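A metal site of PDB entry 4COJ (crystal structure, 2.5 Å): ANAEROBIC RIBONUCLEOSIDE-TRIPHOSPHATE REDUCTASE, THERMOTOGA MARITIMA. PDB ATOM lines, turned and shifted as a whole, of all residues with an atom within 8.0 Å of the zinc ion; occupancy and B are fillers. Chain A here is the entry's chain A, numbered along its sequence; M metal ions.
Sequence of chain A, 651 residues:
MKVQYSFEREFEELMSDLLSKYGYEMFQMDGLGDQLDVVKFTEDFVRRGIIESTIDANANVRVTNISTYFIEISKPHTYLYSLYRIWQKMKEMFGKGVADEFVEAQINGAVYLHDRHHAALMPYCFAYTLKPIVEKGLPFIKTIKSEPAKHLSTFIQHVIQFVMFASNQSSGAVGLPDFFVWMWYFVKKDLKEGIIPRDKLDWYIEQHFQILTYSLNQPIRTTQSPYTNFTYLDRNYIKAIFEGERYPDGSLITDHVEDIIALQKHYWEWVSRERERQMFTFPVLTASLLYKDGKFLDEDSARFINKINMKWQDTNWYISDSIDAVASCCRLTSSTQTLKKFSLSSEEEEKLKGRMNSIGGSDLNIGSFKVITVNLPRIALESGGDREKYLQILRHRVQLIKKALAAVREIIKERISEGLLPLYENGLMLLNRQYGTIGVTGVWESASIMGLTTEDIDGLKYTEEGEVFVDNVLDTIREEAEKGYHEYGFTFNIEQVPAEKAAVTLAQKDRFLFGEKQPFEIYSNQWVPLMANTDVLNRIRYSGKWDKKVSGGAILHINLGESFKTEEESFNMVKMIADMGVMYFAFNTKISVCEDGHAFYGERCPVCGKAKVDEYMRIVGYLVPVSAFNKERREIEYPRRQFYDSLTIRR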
ATOM      1  N   GLU A 276      13.304 -25.656  25.998  1.00  0.00           N
ATOM      2  CA  GLU A 276      12.173 -24.874  25.491  1.00  0.00           C
ATOM      3  C   GLU A 276      12.680 -23.735  24.618  1.00  0.00           C
ATOM      4  O   GLU A 276      12.066 -23.400  23.607  1.00  0.00           O
ATOM      5  CB  GLU A 276      11.328 -24.317  26.628  1.00  0.00           C
ATOM      6  CG  GLU A 276      10.013 -23.693  26.151  1.00  0.00           C
ATOM      7  CD  GLU A 276       9.307 -22.879  27.217  1.00  0.00           C
ATOM      8  OE1 GLU A 276       9.445 -23.214  28.411  1.00  0.00           O
ATOM      9  OE2 GLU A 276       8.605 -21.904  26.858  1.00  0.00           O
ATOM     10  N   ARG A 277      13.795 -23.122  25.014  1.00  0.00           N
ATOM     11  CA  ARG A 277      14.411 -22.066  24.228  1.00  0.00           C
ATOM     12  C   ARG A 277      14.907 -22.614  22.905  1.00  0.00           C
ATOM     13  O   ARG A 277      14.558 -22.125  21.831  1.00  0.00           O
ATOM     14  CB  ARG A 277      15.578 -21.429  24.971  1.00  0.00           C
ATOM     15  CG  ARG A 277      15.189 -20.624  26.188  1.00  0.00           C
ATOM     16  CD  ARG A 277      16.425 -20.240  26.969  1.00  0.00           C
ATOM     17  NE  ARG A 277      16.107 -19.385  28.107  1.00  0.00           N
ATOM     18  CZ  ARG A 277      15.579 -19.817  29.251  1.00  0.00           C
ATOM     19  NH1 ARG A 277      15.287 -21.098  29.418  1.00  0.00           N
ATOM     20  NH2 ARG A 277      15.336 -18.952  30.224  1.00  0.00           N
ATOM     21  N   VAL A 593       8.838 -29.694  17.703  1.00  0.00           N
ATOM     22  CA  VAL A 593       9.624 -28.489  17.473  1.00  0.00           C
ATOM     23  C   VAL A 593       9.060 -27.675  16.328  1.00  0.00           C
ATOM     24  O   VAL A 593       8.377 -28.208  15.445  1.00  0.00           O
ATOM     25  CB  VAL A 593      11.110 -28.809  17.163  1.00  0.00           C
ATOM     26  CG1 VAL A 593      11.821 -29.321  18.407  1.00  0.00           C
ATOM     27  CG2 VAL A 593      11.216 -29.800  16.021  1.00  0.00           C
ATOM     28  N   CYS A 594       9.330 -26.368  16.344  1.00  0.00           N
ATOM     29  CA  CYS A 594       8.977 -25.475  15.253  1.00  0.00           C
ATOM     30  C   CYS A 594      10.235 -25.138  14.470  1.00  0.00           C
ATOM     31  O   CYS A 594      11.301 -25.666  14.753  1.00  0.00           O
ATOM     32  CB  CYS A 594       8.327 -24.194  15.781  1.00  0.00           C
ATOM     33  SG  CYS A 594       9.436 -23.158  16.757  1.00  0.00           S
ATOM     34  N   GLU A 595      10.105 -24.247  13.486  1.00  0.00           N
ATOM     35  CA  GLU A 595      11.244 -23.901  12.638  1.00  0.00           C
ATOM     36  C   GLU A 595      12.263 -23.028  13.353  1.00  0.00           C
ATOM     37  O   GLU A 595      13.340 -22.755  12.822  1.00  0.00           O
ATOM     38  CB  GLU A 595      10.765 -23.198  11.367  1.00  0.00           C
ATOM     39  CG  GLU A 595      10.086 -21.856  11.599  1.00  0.00           C
ATOM     40  CD  GLU A 595       9.599 -21.213  10.311  1.00  0.00           C
ATOM     41  OE1 GLU A 595      10.032 -21.671   9.220  1.00  0.00           O
ATOM     42  OE2 GLU A 595       8.803 -20.265  10.384  1.00  0.00           O
ATOM     43  N   ASP A 596      11.932 -22.592  14.567  1.00  0.00           N
ATOM     44  CA  ASP A 596      12.820 -21.754  15.359  1.00  0.00           C
ATOM     45  C   ASP A 596      13.547 -22.550  16.453  1.00  0.00           C
ATOM     46  O   ASP A 596      14.443 -22.021  17.113  1.00  0.00           O
ATOM     47  CB  ASP A 596      12.042 -20.588  15.977  1.00  0.00           C
ATOM     48  CG  ASP A 596      11.490 -19.633  14.927  1.00  0.00           C
ATOM     49  OD1 ASP A 596      11.939 -19.711  13.762  1.00  0.00           O
ATOM     50  OD2 ASP A 596      10.614 -18.808  15.265  1.00  0.00           O
ATOM     51  N   GLY A 597      13.161 -23.806  16.638  1.00  0.00           N
ATOM     52  CA  GLY A 597      13.877 -24.703  17.538  1.00  0.00           C
ATOM     53  C   GLY A 597      13.304 -24.801  18.941  1.00  0.00           C
ATOM     54  O   GLY A 597      13.936 -25.370  19.834  1.00  0.00           O
ATOM     55  N   HIS A 598      12.116 -24.253  19.147  1.00  0.00           N
ATOM     56  CA  HIS A 598      11.454 -24.360  20.438  1.00  0.00           C
ATOM     57  C   HIS A 598      11.035 -25.799  20.704  1.00  0.00           C
ATOM     58  O   HIS A 598      10.444 -26.431  19.843  1.00  0.00           O
ATOM     59  CB  HIS A 598      10.234 -23.447  20.504  1.00  0.00           C
ATOM     60  CG  HIS A 598      10.534 -22.006  20.257  1.00  0.00           C
ATOM     61  ND1 HIS A 598       9.639 -21.148  19.663  1.00  0.00           N
ATOM     62  CD2 HIS A 598      11.640 -21.267  20.532  1.00  0.00           C
ATOM     63  CE1 HIS A 598      10.169 -19.945  19.572  1.00  0.00           C
ATOM     64  NE2 HIS A 598      11.380 -19.989  20.096  1.00  0.00           N
ATOM     65  N   ALA A 599      11.352 -26.311  21.888  1.00  0.00           N
ATOM     66  CA  ALA A 599      10.873 -27.625  22.313  1.00  0.00           C
ATOM     67  C   ALA A 599       9.522 -27.504  23.018  1.00  0.00           C
ATOM     68  O   ALA A 599       9.299 -26.580  23.788  1.00  0.00           O
ATOM     69  CB  ALA A 599      11.869 -28.305  23.219  1.00  0.00           C
ATOM     70  N   PHE A 600       8.633 -28.444  22.733  1.00  0.00           N
ATOM     71  CA  PHE A 600       7.320 -28.485  23.374  1.00  0.00           C
ATOM     72  C   PHE A 600       6.611 -29.790  23.021  1.00  0.00           C
ATOM     73  O   PHE A 600       7.131 -30.603  22.272  1.00  0.00           O
ATOM     74  CB  PHE A 600       6.468 -27.290  22.938  1.00  0.00           C
ATOM     75  CG  PHE A 600       6.278 -27.182  21.454  1.00  0.00           C
ATOM     76  CD1 PHE A 600       7.224 -26.551  20.668  1.00  0.00           C
ATOM     77  CD2 PHE A 600       5.159 -27.708  20.850  1.00  0.00           C
ATOM     78  CE1 PHE A 600       7.055 -26.448  19.302  1.00  0.00           C
ATOM     79  CE2 PHE A 600       4.980 -27.612  19.476  1.00  0.00           C
ATOM     80  CZ  PHE A 600       5.933 -26.979  18.706  1.00  0.00           C
ATOM     81  N   ARG A 604       1.195 -27.191  18.383  1.00  0.00           N
ATOM     82  CA  ARG A 604       1.457 -25.756  18.404  1.00  0.00           C
ATOM     83  C   ARG A 604       2.547 -25.397  19.413  1.00  0.00           C
ATOM     84  O   ARG A 604       2.614 -25.972  20.501  1.00  0.00           O
ATOM     85  CB  ARG A 604       0.183 -24.984  18.746  1.00  0.00           C
ATOM     86  CG  ARG A 604      -0.850 -24.997  17.643  1.00  0.00           C
ATOM     87  CD  ARG A 604      -0.443 -24.094  16.493  1.00  0.00           C
ATOM     88  NE  ARG A 604      -0.294 -22.701  16.931  1.00  0.00           N
ATOM     89  CZ  ARG A 604      -1.318 -21.878  17.149  1.00  0.00           C
ATOM     90  NH1 ARG A 604      -2.562 -22.305  16.985  1.00  0.00           N
ATOM     91  NH2 ARG A 604      -1.089 -20.632  17.535  1.00  0.00           N
ATOM     92  N   CYS A 605       3.385 -24.429  19.051  1.00  0.00           N
ATOM     93  CA  CYS A 605       4.453 -23.972  19.928  1.00  0.00           C
ATOM     94  C   CYS A 605       3.890 -23.024  20.985  1.00  0.00           C
ATOM     95  O   CYS A 605       3.154 -22.088  20.650  1.00  0.00           O
ATOM     96  CB  CYS A 605       5.545 -23.277  19.113  1.00  0.00           C
ATOM     97  SG  CYS A 605       6.982 -22.751  20.073  1.00  0.00           S
ATOM     98  N   PRO A 606       4.211 -23.258  22.274  1.00  0.00           N
ATOM     99  CA  PRO A 606       3.711 -22.369  23.328  1.00  0.00           C
ATOM    100  C   PRO A 606       4.600 -21.150  23.531  1.00  0.00           C
ATOM    101  O   PRO A 606       4.371 -20.370  24.468  1.00  0.00           O
ATOM    102  CB  PRO A 606       3.733 -23.267  24.566  1.00  0.00           C
ATOM    103  CG  PRO A 606       4.905 -24.165  24.329  1.00  0.00           C
ATOM    104  CD  PRO A 606       4.968 -24.392  22.839  1.00  0.00           C
ATOM    105  N   VAL A 607       5.611 -20.990  22.680  1.00  0.00           N
ATOM    106  CA  VAL A 607       6.547 -19.883  22.779  1.00  0.00           C
ATOM    107  C   VAL A 607       6.222 -18.797  21.759  1.00  0.00           C
ATOM    108  O   VAL A 607       6.066 -17.629  22.113  1.00  0.00           O
ATOM    109  CB  VAL A 607       8.007 -20.359  22.583  1.00  0.00           C
ATOM    110  CG1 VAL A 607       8.993 -19.211  22.764  1.00  0.00           C
ATOM    111  CG2 VAL A 607       8.325 -21.488  23.560  1.00  0.00           C
ATOM    112  N   CYS A 608       6.109 -19.205  20.498  1.00  0.00           N
ATOM    113  CA  CYS A 608       5.904 -18.260  19.396  1.00  0.00           C
ATOM    114  C   CYS A 608       4.588 -18.506  18.661  1.00  0.00           C
ATOM    115  O   CYS A 608       4.132 -17.658  17.901  1.00  0.00           O
ATOM    116  CB  CYS A 608       7.072 -18.356  18.401  1.00  0.00           C
ATOM    117  SG  CYS A 608       7.242 -19.973  17.617  1.00  0.00           S
ATOM    118  N   GLY A 609       3.989 -19.666  18.890  1.00  0.00           N
ATOM    119  CA  GLY A 609       2.719 -20.011  18.270  1.00  0.00           C
ATOM    120  C   GLY A 609       2.881 -20.726  16.940  1.00  0.00           C
ATOM    121  O   GLY A 609       1.896 -21.183  16.354  1.00  0.00           O
ATOM    122  N   LYS A 610       4.112 -20.814  16.446  1.00  0.00           N
ATOM    123  CA  LYS A 610       4.378 -21.529  15.204  1.00  0.00           C
ATOM    124  C   LYS A 610       4.082 -23.010  15.366  1.00  0.00           C
ATOM    125  O   LYS A 610       4.457 -23.622  16.371  1.00  0.00           O
ATOM    126  CB  LYS A 610       5.839 -21.322  14.762  1.00  0.00           C
ATOM    127  CG  LYS A 610       6.167 -19.896  14.353  1.00  0.00           C
ATOM    128  CD  LYS A 610       7.591 -19.777  13.828  1.00  0.00           C
ATOM    129  CE  LYS A 610       7.884 -18.384  13.323  1.00  0.00           C
ATOM    130  NZ  LYS A 610       8.665 -18.407  12.044  1.00  0.00           N
ATOM    131  N   ALA A 611       3.406 -23.594  14.379  1.00  0.00           N
ATOM    132  CA  ALA A 611       2.988 -24.987  14.464  1.00  0.00           C
ATOM    133  C   ALA A 611       4.176 -25.932  14.502  1.00  0.00           C
ATOM    134  O   ALA A 611       5.296 -25.566  14.158  1.00  0.00           O
ATOM    135  CB  ALA A 611       2.081 -25.334  13.282  1.00  0.00           C
ATOM    136  N   LYS A 612       3.917 -27.159  14.951  1.00  0.00           N
ATOM    137  CA  LYS A 612       4.913 -28.220  14.918  1.00  0.00           C
ATOM    138  C   LYS A 612       5.303 -28.493  13.469  1.00  0.00           C
ATOM    139  O   LYS A 612       4.475 -28.368  12.569  1.00  0.00           O
ATOM    140  CB  LYS A 612       4.352 -29.483  15.580  1.00  0.00           C
ATOM    141  CG  LYS A 612       5.007 -30.794  15.135  1.00  0.00           C
ATOM    142  CD  LYS A 612       4.326 -31.979  15.790  1.00  0.00           C
ATOM    143  CE  LYS A 612       4.748 -33.270  15.121  1.00  0.00           C
ATOM    144  NZ  LYS A 612       4.356 -34.450  15.925  1.00  0.00           N
HETATM  145 ZN    ZN M   1       8.320 -21.869  18.299  1.00  0.00          ZN
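SG of Cys 608 sits close to N of Lys 610.
SG of Cys 594 sits close to N of Asp 596 (3.4 Å).
SG of Cys 594 lies close to N of Gly 597.
N of Cys 605 sits close to O of Lys 610.
The side-chain sulfur of Cys 605 sits close to the backbone NH of Val 607.
Along chain A the residues within 4 Å of the zinc ion span positions 594 to 608.
A ring nitrogen (ND1) of His 598 is bound to the zinc ion (2.0 Å).
SG of Cys 608 is bound to the zinc ion.
The side-chain sulfur (SG) of Cys 594 is bound to the zinc ion.
SG of Cys 605 binds the zinc ion (2.4 Å).
The zinc ion has four donor atoms within binding distance.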
